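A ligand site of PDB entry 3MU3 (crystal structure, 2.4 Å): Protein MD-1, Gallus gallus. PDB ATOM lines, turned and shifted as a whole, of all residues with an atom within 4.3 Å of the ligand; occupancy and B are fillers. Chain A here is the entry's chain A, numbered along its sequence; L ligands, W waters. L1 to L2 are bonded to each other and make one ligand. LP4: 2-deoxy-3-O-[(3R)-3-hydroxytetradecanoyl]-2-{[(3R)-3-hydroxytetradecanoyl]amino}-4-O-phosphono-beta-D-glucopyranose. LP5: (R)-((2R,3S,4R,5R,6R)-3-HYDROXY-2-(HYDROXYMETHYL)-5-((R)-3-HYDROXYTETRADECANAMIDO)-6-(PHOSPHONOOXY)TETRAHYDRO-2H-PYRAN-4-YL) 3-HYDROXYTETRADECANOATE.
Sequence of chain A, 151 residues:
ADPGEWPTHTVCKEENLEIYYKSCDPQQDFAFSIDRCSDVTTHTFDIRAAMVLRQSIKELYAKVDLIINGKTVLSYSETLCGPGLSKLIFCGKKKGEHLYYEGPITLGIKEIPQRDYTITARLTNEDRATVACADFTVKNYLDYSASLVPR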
ATOM      1  N   ILE A  19      -9.786  12.542  16.209  1.00  0.00           N
ATOM      2  CA  ILE A  19      -8.442  12.327  16.743  1.00  0.00           C
ATOM      3  C   ILE A  19      -8.398  12.358  18.280  1.00  0.00           C
ATOM      4  O   ILE A  19      -8.880  13.311  18.918  1.00  0.00           O
ATOM      5  CB  ILE A  19      -7.449  13.374  16.229  1.00  0.00           C
ATOM      6  CG1 ILE A  19      -7.476  13.409  14.688  1.00  0.00           C
ATOM      7  CG2 ILE A  19      -6.050  13.053  16.739  1.00  0.00           C
ATOM      8  CD1 ILE A  19      -6.316  14.106  14.052  1.00  0.00           C
ATOM      9  N   PHE A  30       0.356  15.433  28.972  1.00  0.00           N
ATOM     10  CA  PHE A  30       0.676  16.703  28.336  1.00  0.00           C
ATOM     11  C   PHE A  30      -0.555  17.275  27.648  1.00  0.00           C
ATOM     12  O   PHE A  30      -1.491  16.563  27.401  1.00  0.00           O
ATOM     13  CB  PHE A  30       1.788  16.507  27.316  1.00  0.00           C
ATOM     14  CG  PHE A  30       1.384  15.717  26.143  1.00  0.00           C
ATOM     15  CD1 PHE A  30       1.536  14.341  26.138  1.00  0.00           C
ATOM     16  CD2 PHE A  30       0.943  16.334  24.997  1.00  0.00           C
ATOM     17  CE1 PHE A  30       1.188  13.600  25.045  1.00  0.00           C
ATOM     18  CE2 PHE A  30       0.578  15.573  23.894  1.00  0.00           C
ATOM     19  CZ  PHE A  30       0.760  14.213  23.903  1.00  0.00           C
ATOM     20  N   PHE A  32      -2.363  19.045  24.296  1.00  0.00           N
ATOM     21  CA  PHE A  32      -2.194  19.140  22.838  1.00  0.00           C
ATOM     22  C   PHE A  32      -3.503  19.537  22.188  1.00  0.00           C
ATOM     23  O   PHE A  32      -4.550  19.105  22.618  1.00  0.00           O
ATOM     24  CB  PHE A  32      -1.705  17.795  22.301  1.00  0.00           C
ATOM     25  CG  PHE A  32      -1.348  17.810  20.858  1.00  0.00           C
ATOM     26  CD1 PHE A  32      -2.345  17.622  19.877  1.00  0.00           C
ATOM     27  CD2 PHE A  32      -0.019  17.833  20.459  1.00  0.00           C
ATOM     28  CE1 PHE A  32      -2.023  17.484  18.551  1.00  0.00           C
ATOM     29  CE2 PHE A  32       0.309  17.776  19.103  1.00  0.00           C
ATOM     30  CZ  PHE A  32      -0.717  17.614  18.137  1.00  0.00           C
ATOM     31  N   ALA A  49       0.785  22.894  22.168  1.00  0.00           N
ATOM     32  CA  ALA A  49       1.202  21.826  23.027  1.00  0.00           C
ATOM     33  C   ALA A  49       1.910  22.410  24.229  1.00  0.00           C
ATOM     34  O   ALA A  49       2.632  23.392  24.068  1.00  0.00           O
ATOM     35  CB  ALA A  49       2.113  20.897  22.295  1.00  0.00           C
ATOM     36  N   ALA A  62      12.535  12.300  17.570  1.00  0.00           N
ATOM     37  CA  ALA A  62      11.190  11.777  17.461  1.00  0.00           C
ATOM     38  C   ALA A  62      11.358  10.442  16.839  1.00  0.00           C
ATOM     39  O   ALA A  62      12.096  10.347  15.837  1.00  0.00           O
ATOM     40  CB  ALA A  62      10.288  12.691  16.541  1.00  0.00           C
ATOM     41  N   VAL A  64       8.336   7.958  15.206  1.00  0.00           N
ATOM     42  CA  VAL A  64       6.926   7.943  14.852  1.00  0.00           C
ATOM     43  C   VAL A  64       6.582   6.586  14.252  1.00  0.00           C
ATOM     44  O   VAL A  64       7.074   6.254  13.185  1.00  0.00           O
ATOM     45  CB  VAL A  64       6.607   9.035  13.807  1.00  0.00           C
ATOM     46  CG1 VAL A  64       5.139   8.954  13.387  1.00  0.00           C
ATOM     47  CG2 VAL A  64       6.964  10.463  14.347  1.00  0.00           C
ATOM     48  N   LEU A  74       4.697   1.200   9.543  1.00  0.00           N
ATOM     49  CA  LEU A  74       5.700   2.223   9.209  1.00  0.00           C
ATOM     50  C   LEU A  74       6.412   2.665  10.479  1.00  0.00           C
ATOM     51  O   LEU A  74       5.756   2.973  11.515  1.00  0.00           O
ATOM     52  CB  LEU A  74       5.048   3.450   8.566  1.00  0.00           C
ATOM     53  CG  LEU A  74       5.848   4.775   8.486  1.00  0.00           C
ATOM     54  CD1 LEU A  74       6.726   4.650   7.294  1.00  0.00           C
ATOM     55  CD2 LEU A  74       4.948   6.010   8.360  1.00  0.00           C
ATOM     56  N   TYR A  76       9.434   5.650  11.589  1.00  0.00           N
ATOM     57  CA  TYR A  76      10.153   6.842  11.075  1.00  0.00           C
ATOM     58  C   TYR A  76      10.858   7.526  12.242  1.00  0.00           C
ATOM     59  O   TYR A  76      10.195   7.888  13.244  1.00  0.00           O
ATOM     60  CB  TYR A  76       9.181   7.842  10.393  1.00  0.00           C
ATOM     61  CG  TYR A  76       9.750   9.239  10.155  1.00  0.00           C
ATOM     62  CD1 TYR A  76      10.665   9.472   9.121  1.00  0.00           C
ATOM     63  CD2 TYR A  76       9.302  10.337  10.881  1.00  0.00           C
ATOM     64  CE1 TYR A  76      11.195  10.759   8.869  1.00  0.00           C
ATOM     65  CE2 TYR A  76       9.788  11.617  10.619  1.00  0.00           C
ATOM     66  CZ  TYR A  76      10.750  11.840   9.623  1.00  0.00           C
ATOM     67  OH  TYR A  76      11.247  13.127   9.328  1.00  0.00           O
ATOM     68  N   GLU A  78      13.355  10.954  13.275  1.00  0.00           N
ATOM     69  CA  GLU A  78      13.904  12.286  12.946  1.00  0.00           C
ATOM     70  C   GLU A  78      14.617  12.879  14.139  1.00  0.00           C
ATOM     71  O   GLU A  78      14.106  12.773  15.225  1.00  0.00           O
ATOM     72  CB  GLU A  78      12.754  13.235  12.572  1.00  0.00           C
ATOM     73  CG  GLU A  78      13.137  14.514  11.854  1.00  0.00           C
ATOM     74  CD  GLU A  78      11.943  15.406  11.658  1.00  0.00           C
ATOM     75  OE1 GLU A  78      10.861  15.115  12.202  1.00  0.00           O
ATOM     76  OE2 GLU A  78      12.059  16.352  10.864  1.00  0.00           O
ATOM     77  N   LEU A  80      15.327  16.246  16.046  1.00  0.00           N
ATOM     78  CA  LEU A  80      14.694  17.568  16.196  1.00  0.00           C
ATOM     79  C   LEU A  80      15.623  18.582  16.910  1.00  0.00           C
ATOM     80  O   LEU A  80      15.573  19.752  16.571  1.00  0.00           O
ATOM     81  CB  LEU A  80      13.356  17.476  16.933  1.00  0.00           C
ATOM     82  CG  LEU A  80      12.170  16.801  16.225  1.00  0.00           C
ATOM     83  CD1 LEU A  80      11.018  16.608  17.248  1.00  0.00           C
ATOM     84  CD2 LEU A  80      11.696  17.622  15.033  1.00  0.00           C
ATOM     85  N   LYS A  87      15.789  22.179  15.194  1.00  0.00           N
ATOM     86  CA  LYS A  87      14.552  22.382  14.413  1.00  0.00           C
ATOM     87  C   LYS A  87      13.425  23.029  15.255  1.00  0.00           C
ATOM     88  O   LYS A  87      12.271  23.066  14.822  1.00  0.00           O
ATOM     89  CB  LYS A  87      14.060  21.020  13.872  1.00  0.00           C
ATOM     90  CG  LYS A  87      14.256  20.806  12.365  1.00  0.00           C
ATOM     91  CD  LYS A  87      13.891  19.386  11.937  1.00  0.00           C
ATOM     92  CE  LYS A  87      14.842  18.816  10.857  1.00  0.00           C
ATOM     93  NZ  LYS A  87      15.137  17.325  11.120  1.00  0.00           N
ATOM     94  N   LEU A  88      13.757  23.521  16.441  1.00  0.00           N
ATOM     95  CA  LEU A  88      12.776  23.932  17.431  1.00  0.00           C
ATOM     96  C   LEU A  88      13.442  24.972  18.315  1.00  0.00           C
ATOM     97  O   LEU A  88      14.509  24.729  18.840  1.00  0.00           O
ATOM     98  CB  LEU A  88      12.338  22.748  18.289  1.00  0.00           C
ATOM     99  CG  LEU A  88      11.385  21.732  17.654  1.00  0.00           C
ATOM    100  CD1 LEU A  88      11.451  20.431  18.425  1.00  0.00           C
ATOM    101  CD2 LEU A  88       9.965  22.275  17.613  1.00  0.00           C
ATOM    102  N   PHE A  90      12.986  25.931  21.079  1.00  0.00           N
ATOM    103  CA  PHE A  90      13.029  25.482  22.461  1.00  0.00           C
ATOM    104  C   PHE A  90      13.893  24.214  22.706  1.00  0.00           C
ATOM    105  O   PHE A  90      13.893  23.666  23.813  1.00  0.00           O
ATOM    106  CB  PHE A  90      11.596  25.247  22.957  1.00  0.00           C
ATOM    107  CG  PHE A  90      10.851  24.118  22.238  1.00  0.00           C
ATOM    108  CD1 PHE A  90      11.029  22.784  22.621  1.00  0.00           C
ATOM    109  CD2 PHE A  90       9.863  24.402  21.299  1.00  0.00           C
ATOM    110  CE1 PHE A  90      10.303  21.763  22.008  1.00  0.00           C
ATOM    111  CE2 PHE A  90       9.132  23.370  20.695  1.00  0.00           C
ATOM    112  CZ  PHE A  90       9.342  22.057  21.063  1.00  0.00           C
ATOM    113  N   TYR A 101       4.695  25.081  22.786  1.00  0.00           N
ATOM    114  CA  TYR A 101       4.746  25.222  21.359  1.00  0.00           C
ATOM    115  C   TYR A 101       3.355  25.636  20.848  1.00  0.00           C
ATOM    116  O   TYR A 101       2.347  24.987  21.110  1.00  0.00           O
ATOM    117  CB  TYR A 101       5.211  23.902  20.719  1.00  0.00           C
ATOM    118  CG  TYR A 101       5.464  24.001  19.210  1.00  0.00           C
ATOM    119  CD1 TYR A 101       6.578  24.682  18.717  1.00  0.00           C
ATOM    120  CD2 TYR A 101       4.558  23.455  18.280  1.00  0.00           C
ATOM    121  CE1 TYR A 101       6.790  24.811  17.350  1.00  0.00           C
ATOM    122  CE2 TYR A 101       4.807  23.539  16.903  1.00  0.00           C
ATOM    123  CZ  TYR A 101       5.923  24.208  16.445  1.00  0.00           C
ATOM    124  OH  TYR A 101       6.144  24.318  15.083  1.00  0.00           O
ATOM    125  N   PRO A 104       3.032  25.489  13.385  1.00  0.00           N
ATOM    126  CA  PRO A 104       2.651  24.431  12.471  1.00  0.00           C
ATOM    127  C   PRO A 104       3.506  23.211  12.660  1.00  0.00           C
ATOM    128  O   PRO A 104       4.717  23.318  12.840  1.00  0.00           O
ATOM    129  CB  PRO A 104       2.908  25.051  11.095  1.00  0.00           C
ATOM    130  CG  PRO A 104       4.064  25.955  11.325  1.00  0.00           C
ATOM    131  CD  PRO A 104       3.891  26.481  12.736  1.00  0.00           C
ATOM    132  N   ILE A 105       2.893  22.039  12.622  1.00  0.00           N
ATOM    133  CA  ILE A 105       3.522  20.903  11.994  1.00  0.00           C
ATOM    134  C   ILE A 105       3.450  21.041  10.467  1.00  0.00           C
ATOM    135  O   ILE A 105       2.371  20.925   9.881  1.00  0.00           O
ATOM    136  CB  ILE A 105       2.857  19.599  12.383  1.00  0.00           C
ATOM    137  CG1 ILE A 105       3.185  19.263  13.848  1.00  0.00           C
ATOM    138  CG2 ILE A 105       3.361  18.499  11.438  1.00  0.00           C
ATOM    139  CD1 ILE A 105       2.492  17.927  14.382  1.00  0.00           C
ATOM    140  N   THR A 106       4.602  21.254   9.824  1.00  0.00           N
ATOM    141  CA  THR A 106       4.734  20.972   8.398  1.00  0.00           C
ATOM    142  C   THR A 106       4.994  19.481   8.129  1.00  0.00           C
ATOM    143  O   THR A 106       4.801  18.644   8.996  1.00  0.00           O
ATOM    144  CB  THR A 106       5.845  21.818   7.748  1.00  0.00           C
ATOM    145  OG1 THR A 106       6.334  22.830   8.670  1.00  0.00           O
ATOM    146  CG2 THR A 106       5.336  22.468   6.422  1.00  0.00           C
ATOM    147  N   LEU A 107       5.285  19.129   6.880  1.00  0.00           N
ATOM    148  CA  LEU A 107       5.004  17.790   6.387  1.00  0.00           C
ATOM    149  C   LEU A 107       5.511  17.633   4.933  1.00  0.00           C
ATOM    150  O   LEU A 107       5.114  18.395   4.048  1.00  0.00           O
ATOM    151  CB  LEU A 107       3.499  17.495   6.506  1.00  0.00           C
ATOM    152  N   GLY A 108       6.603  16.869   4.784  1.00  0.00           N
ATOM    153  CA  GLY A 108       6.962  16.211   3.526  1.00  0.00           C
ATOM    154  C   GLY A 108       5.898  15.294   2.944  1.00  0.00           C
ATOM    155  O   GLY A 108       5.719  15.280   1.726  1.00  0.00           O
ATOM    156  N   ILE A 109       5.180  14.569   3.809  1.00  0.00           N
ATOM    157  CA  ILE A 109       3.867  13.964   3.442  1.00  0.00           C
ATOM    158  C   ILE A 109       2.840  15.091   3.215  1.00  0.00           C
ATOM    159  O   ILE A 109       2.828  16.057   3.995  1.00  0.00           O
ATOM    160  CB  ILE A 109       3.303  13.011   4.541  1.00  0.00           C
ATOM    161  N   ILE A 119      -1.048   6.359  15.721  1.00  0.00           N
ATOM    162  CA  ILE A 119       0.306   6.854  15.564  1.00  0.00           C
ATOM    163  C   ILE A 119       0.845   6.930  16.953  1.00  0.00           C
ATOM    164  O   ILE A 119       0.293   7.666  17.772  1.00  0.00           O
ATOM    165  CB  ILE A 119       0.325   8.269  14.993  1.00  0.00           C
ATOM    166  CG1 ILE A 119      -0.024   8.245  13.519  1.00  0.00           C
ATOM    167  CG2 ILE A 119       1.719   8.877  15.164  1.00  0.00           C
ATOM    168  CD1 ILE A 119      -0.111   9.626  12.916  1.00  0.00           C
ATOM    169  N   ALA A 121       3.997   8.353  18.877  1.00  0.00           N
ATOM    170  CA  ALA A 121       5.004   9.400  18.680  1.00  0.00           C
ATOM    171  C   ALA A 121       5.761   9.496  19.963  1.00  0.00           C
ATOM    172  O   ALA A 121       5.253   9.978  20.978  1.00  0.00           O
ATOM    173  CB  ALA A 121       4.346  10.771  18.363  1.00  0.00           C
ATOM    174  N   ALA A 132       8.651  12.583  26.000  1.00  0.00           N
ATOM    175  CA  ALA A 132       7.186  12.555  25.799  1.00  0.00           C
ATOM    176  C   ALA A 132       6.900  11.404  24.866  1.00  0.00           C
ATOM    177  O   ALA A 132       7.802  10.951  24.159  1.00  0.00           O
ATOM    178  CB  ALA A 132       6.679  13.851  25.186  1.00  0.00           C
ATOM    179  N   CYS A 133       5.703  10.860  25.011  1.00  0.00           N
ATOM    180  CA  CYS A 133       5.221   9.706  24.253  1.00  0.00           C
ATOM    181  C   CYS A 133       3.673   9.842  24.142  1.00  0.00           C
ATOM    182  O   CYS A 133       2.997   9.921  25.150  1.00  0.00           O
ATOM    183  CB  CYS A 133       5.588   8.436  25.005  1.00  0.00           C
ATOM    184  SG  CYS A 133       5.058   6.822  24.243  1.00  0.00           S
ATOM    185  N   ALA A 134       3.139   9.840  22.928  1.00  0.00           N
ATOM    186  CA  ALA A 134       1.685   9.825  22.703  1.00  0.00           C
ATOM    187  C   ALA A 134       1.319   8.604  21.826  1.00  0.00           C
ATOM    188  O   ALA A 134       2.080   8.291  20.895  1.00  0.00           O
ATOM    189  CB  ALA A 134       1.238  11.167  22.003  1.00  0.00           C
ATOM    190  N   PHE A 136      -1.617   8.447  19.460  1.00  0.00           N
ATOM    191  CA  PHE A 136      -2.774   9.115  18.813  1.00  0.00           C
ATOM    192  C   PHE A 136      -3.671   8.122  18.084  1.00  0.00           C
ATOM    193  O   PHE A 136      -3.157   7.240  17.374  1.00  0.00           O
ATOM    194  CB  PHE A 136      -2.305  10.133  17.784  1.00  0.00           C
ATOM    195  CG  PHE A 136      -1.627  11.315  18.360  1.00  0.00           C
ATOM    196  CD1 PHE A 136      -2.353  12.433  18.706  1.00  0.00           C
ATOM    197  CD2 PHE A 136      -0.266  11.372  18.450  1.00  0.00           C
ATOM    198  CE1 PHE A 136      -1.730  13.570  19.172  1.00  0.00           C
ATOM    199  CE2 PHE A 136       0.382  12.587  18.823  1.00  0.00           C
ATOM    200  CZ  PHE A 136      -0.354  13.634  19.243  1.00  0.00           C
ATOM    201  N   VAL A 138      -6.430   7.828  15.254  1.00  0.00           N
ATOM    202  CA  VAL A 138      -6.995   8.557  14.134  1.00  0.00           C
ATOM    203  C   VAL A 138      -8.128   7.786  13.448  1.00  0.00           C
ATOM    204  O   VAL A 138      -8.035   6.574  13.191  1.00  0.00           O
ATOM    205  CB  VAL A 138      -5.913   8.910  13.154  1.00  0.00           C
ATOM    206  CG1 VAL A 138      -6.494   9.878  12.065  1.00  0.00           C
ATOM    207  CG2 VAL A 138      -4.735   9.517  13.906  1.00  0.00           C
HETATM  208  C1  LP4 L   1      11.245  21.332   8.439  1.00  0.00           C
HETATM  209  C2  LP4 L   1      10.586  21.187   9.840  1.00  0.00           C
HETATM  210  N2  LP4 L   1       9.408  20.293   9.798  1.00  0.00           N
HETATM  211  C3  LP4 L   1      10.241  22.538  10.435  1.00  0.00           C
HETATM  212  O3  LP4 L   1       9.842  22.247  11.781  1.00  0.00           O
HETATM  213  C4  LP4 L   1      11.496  23.384  10.536  1.00  0.00           C
HETATM  214  O4  LP4 L   1      11.106  24.665  10.937  1.00  0.00           O
HETATM  215  C5  LP4 L   1      12.222  23.539   9.198  1.00  0.00           C
HETATM  216  O5  LP4 L   1      12.342  22.325   8.350  1.00  0.00           O
HETATM  217  C6  LP4 L   1      13.610  24.085   9.647  1.00  0.00           C
HETATM  218  O6  LP4 L   1      14.564  23.029   9.821  1.00  0.00           O
HETATM  219  C7  LP4 L   1       9.472  19.069  10.329  1.00  0.00           C
HETATM  220  O7  LP4 L   1      10.454  18.664  10.975  1.00  0.00           O
HETATM  221  C8  LP4 L   1       8.173  18.225  10.276  1.00  0.00           C
HETATM  222  C16 LP4 L   1       8.358  16.956  11.133  1.00  0.00           C
HETATM  223  C17 LP4 L   1       7.133  16.702  11.991  1.00  0.00           C
HETATM  224  C18 LP4 L   1       7.346  15.437  12.834  1.00  0.00           C
HETATM  225  C19 LP4 L   1       6.806  15.632  14.254  1.00  0.00           C
HETATM  226  C20 LP4 L   1       7.708  14.939  15.287  1.00  0.00           C
HETATM  227  C21 LP4 L   1       6.831  14.177  16.252  1.00  0.00           C
HETATM  228  C22 LP4 L   1       6.041  15.141  17.122  1.00  0.00           C
HETATM  229  C23 LP4 L   1       4.590  14.679  17.297  1.00  0.00           C
HETATM  230  C24 LP4 L   1       3.592  15.718  16.790  1.00  0.00           C
HETATM  231  C25 LP4 L   1       2.247  15.543  17.506  1.00  0.00           C
HETATM  232  C28 LP4 L   1       8.580  22.728  12.055  1.00  0.00           C
HETATM  233  C29 LP4 L   1       7.606  21.844  12.933  1.00  0.00           C
HETATM  234  C30 LP4 L   1       8.402  21.050  14.006  1.00  0.00           C
HETATM  235  C31 LP4 L   1       7.645  20.975  15.339  1.00  0.00           C
HETATM  236  C32 LP4 L   1       7.719  19.615  16.055  1.00  0.00           C
HETATM  237  C33 LP4 L   1       6.591  19.501  17.117  1.00  0.00           C
HETATM  238  C34 LP4 L   1       7.087  19.823  18.528  1.00  0.00           C
HETATM  239  C35 LP4 L   1       6.647  18.742  19.535  1.00  0.00           C
HETATM  240  C36 LP4 L   1       5.583  19.219  20.554  1.00  0.00           C
HETATM  241  C37 LP4 L   1       4.998  18.037  21.399  1.00  0.00           C
HETATM  242  C38 LP4 L   1       4.254  16.984  20.535  1.00  0.00           C
HETATM  243  C39 LP4 L   1       3.770  15.767  21.339  1.00  0.00           C
HETATM  244  C40 LP4 L   1       4.440  14.406  20.974  1.00  0.00           C
HETATM  245  C41 LP4 L   1       4.231  13.334  22.082  1.00  0.00           C
HETATM  246  O42 LP4 L   1       8.300  23.893  11.717  1.00  0.00           O
HETATM  247  O43 LP4 L   1       8.757  19.720  13.526  1.00  0.00           O
HETATM  248  O44 LP4 L   1       8.644  15.762  10.359  1.00  0.00           O
HETATM  249  P45 LP4 L   1      11.465  25.357  12.310  1.00  0.00           P
HETATM  250  O46 LP4 L   1      12.989  25.030  12.650  1.00  0.00           O
HETATM  251  O47 LP4 L   1      10.632  24.681  13.534  1.00  0.00           O
HETATM  252  O48 LP4 L   1      11.100  26.775  12.224  1.00  0.00           O
HETATM  253  O48 LP5 L   2      15.964  15.703   5.212  1.00  0.00           O
HETATM  254  P45 LP5 L   2      15.270  17.000   4.902  1.00  0.00           P
HETATM  255  O46 LP5 L   2      15.967  18.343   5.579  1.00  0.00           O
HETATM  256  O47 LP5 L   2      15.160  17.349   3.323  1.00  0.00           O
HETATM  257  O1  LP5 L   2      13.746  16.883   5.474  1.00  0.00           O
HETATM  258  C1  LP5 L   2      13.509  16.689   6.868  1.00  0.00           C
HETATM  259  C2  LP5 L   2      12.584  15.497   7.128  1.00  0.00           C
HETATM  260  N2  LP5 L   2      13.136  14.398   6.332  1.00  0.00           N
HETATM  261  C7  LP5 L   2      13.671  13.332   6.920  1.00  0.00           C
HETATM  262  C8  LP5 L   2      14.240  12.221   6.001  1.00  0.00           C
HETATM  263  C16 LP5 L   2      13.763  12.293   4.555  1.00  0.00           C
HETATM  264  O44 LP5 L   2      13.954  13.643   4.092  1.00  0.00           O
HETATM  265  C17 LP5 L   2      12.277  11.980   4.414  1.00  0.00           C
HETATM  266  C18 LP5 L   2      11.886  10.572   4.912  1.00  0.00           C
HETATM  267  C19 LP5 L   2      10.455  10.203   4.427  1.00  0.00           C
HETATM  268  C20 LP5 L   2       9.405  10.458   5.519  1.00  0.00           C
HETATM  269  C21 LP5 L   2       8.075   9.752   5.198  1.00  0.00           C
HETATM  270  C22 LP5 L   2       7.257   9.591   6.509  1.00  0.00           C
HETATM  271  C23 LP5 L   2       5.761   9.939   6.352  1.00  0.00           C
HETATM  272  C24 LP5 L   2       5.060   9.774   7.727  1.00  0.00           C
HETATM  273  C25 LP5 L   2       3.541   9.539   7.660  1.00  0.00           C
HETATM  274  C26 LP5 L   2       3.087   8.651   8.857  1.00  0.00           C
HETATM  275  C27 LP5 L   2       2.463   9.494   9.989  1.00  0.00           C
HETATM  276  O7  LP5 L   2      13.676  13.189   8.128  1.00  0.00           O
HETATM  277  C3  LP5 L   2      11.143  15.765   6.635  1.00  0.00           C
HETATM  278  C4  LP5 L   2      10.730  17.240   6.840  1.00  0.00           C
HETATM  279  C5  LP5 L   2      11.827  18.226   6.386  1.00  0.00           C
HETATM  280  O5  LP5 L   2      12.923  17.903   7.260  1.00  0.00           O
HETATM  281  C6  LP5 L   2      11.477  19.716   6.649  1.00  0.00           C
HETATM  282  O6  LP5 L   2      11.666  20.001   8.044  1.00  0.00           O
HETATM  283  O4  LP5 L   2       9.524  17.528   6.133  1.00  0.00           O
HETATM  284  O3  LP5 L   2      10.171  14.737   7.173  1.00  0.00           O
HETATM  285  C28 LP5 L   2       9.000  14.637   6.421  1.00  0.00           C
HETATM  286  O42 LP5 L   2       9.024  14.229   5.253  1.00  0.00           O
HETATM  287  C29 LP5 L   2       7.627  14.957   7.064  1.00  0.00           C
HETATM  288  C30 LP5 L   2       7.447  14.099   8.307  1.00  0.00           C
HETATM  289  O43 LP5 L   2       7.841  12.773   7.985  1.00  0.00           O
HETATM  290  C31 LP5 L   2       5.999  14.174   8.812  1.00  0.00           C
HETATM  291  C32 LP5 L   2       5.453  12.844   9.418  1.00  0.00           C
HETATM  292  C33 LP5 L   2       5.159  12.934  10.919  1.00  0.00           C
HETATM  293  C34 LP5 L   2       3.675  12.753  11.247  1.00  0.00           C
HETATM  294  C35 LP5 L   2       3.404  13.312  12.663  1.00  0.00           C
HETATM  295  C36 LP5 L   2       1.934  13.738  12.902  1.00  0.00           C
HETATM  296  C37 LP5 L   2       1.648  13.612  14.419  1.00  0.00           C
HETATM  297  C38 LP5 L   2       0.305  14.246  14.820  1.00  0.00           C
HETATM  298  C39 LP5 L   2      -0.845  13.315  14.442  1.00  0.00           C
HETATM  299  C40 LP5 L   2      -2.172  13.833  14.997  1.00  0.00           C
HETATM  300  C41 LP5 L   2      -3.065  12.625  15.234  1.00  0.00           C
HETATM  301  O   HOH W   1      17.520  22.237   8.747  1.00  0.00           O
HETATM  302  O   HOH W   2      13.703  16.056   1.265  1.00  0.00           O
HETATM  303  O   HOH W   3       8.574  26.829  10.275  1.00  0.00           O
HETATM  304  O   HOH W   4      15.110  11.314   9.347  1.00  0.00           O
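An oxygen (O47) of LP4 L1 lies close to the backbone carbonyl oxygen (O) of Lys 87 (2.6 Å).
The side-chain hydroxyl of Tyr 76 is in hydrogen-bond range of an oxygen (O7) of LP5 L2, 2.7 Å away.
The side-chain carboxylate (OE1) of Glu 78 is in hydrogen-bond range of an oxygen (O44) of LP4 L1, at 3.0 Å.
An oxygen (O4) of LP5 L2 sits close to the backbone NH (N) of Gly 108 (3.3 Å).
The side-chain carboxylate (OE2) of Glu 78 lies within salt-bridge range of the side-chain amino group (NZ) of Lys 87 (3.2 Å).
N of Lys 87 sits at hydrogen-bond distance from O of Leu 80, at 2.8 Å.
The backbone carbonyl oxygen (O) of Tyr 76 is in hydrogen-bond range of the backbone NH (N) of Val 64 (2.7 Å).
The backbone carbonyl oxygen of Glu 78 lies within hydrogen-bond range of the backbone NH of Ala 62, 2.9 Å away.
The backbone carbonyl oxygen (O) of Pro 104 lies within hydrogen-bond range of the side-chain hydroxyl (OH) of Tyr 101 (2.8 Å).
The backbone NH of Phe 136 is in hydrogen-bond range of the backbone carbonyl oxygen of Ile 119 (2.7 Å).
The backbone NH (N) of Ala 49 sits at hydrogen-bond distance from the backbone carbonyl oxygen (O) of Tyr 101, 2.8 Å away.
N of Ala 121 lies within hydrogen-bond range of O of Ala 134 (2.8 Å).
Ile 19 touches the ligand.
CE2 of Phe 32 touches C25 of LP4 L1, at 3.4 Å.
Ala 62 touches the ligand.
Leu 74 touches the ligand.
CD2 of Leu 80 touches O43 of LP4 L1, 3.9 Å away.
CD2 of Leu 88 touches C31 of LP4 L1, 3.5 Å away.
OH of Tyr 101 touches C29 of LP4 L1, 3.6 Å away.
Pro 104 touches the ligand.
CD1 of Ile 105 touches C24 of LP4 L1, at 3.4 Å.
Thr 106 touches the ligand.
CA of Leu 107 touches C29 of LP5 L2, 3.9 Å away.
CD1 of Ile 119 touches C27 of LP5 L2, 3.9 Å away.
O of Ala 121 touches C41 of LP4 L1 (3.7 Å).
CB of Ala 132 touches C41 of LP4 L1, at 3.99 Å.
CB of Ala 134 touches C41 of LP4 L1, at 3.7 Å.
CD1 of Phe 136 touches C41 of LP5 L2, 3.5 Å away.
Val 138 touches the ligand.
Of the 27 residues printed, 21 come within 4 Å of the ligand.
The nearest printed residue that does not touch the ligand is Phe 30 (4.02 Å).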
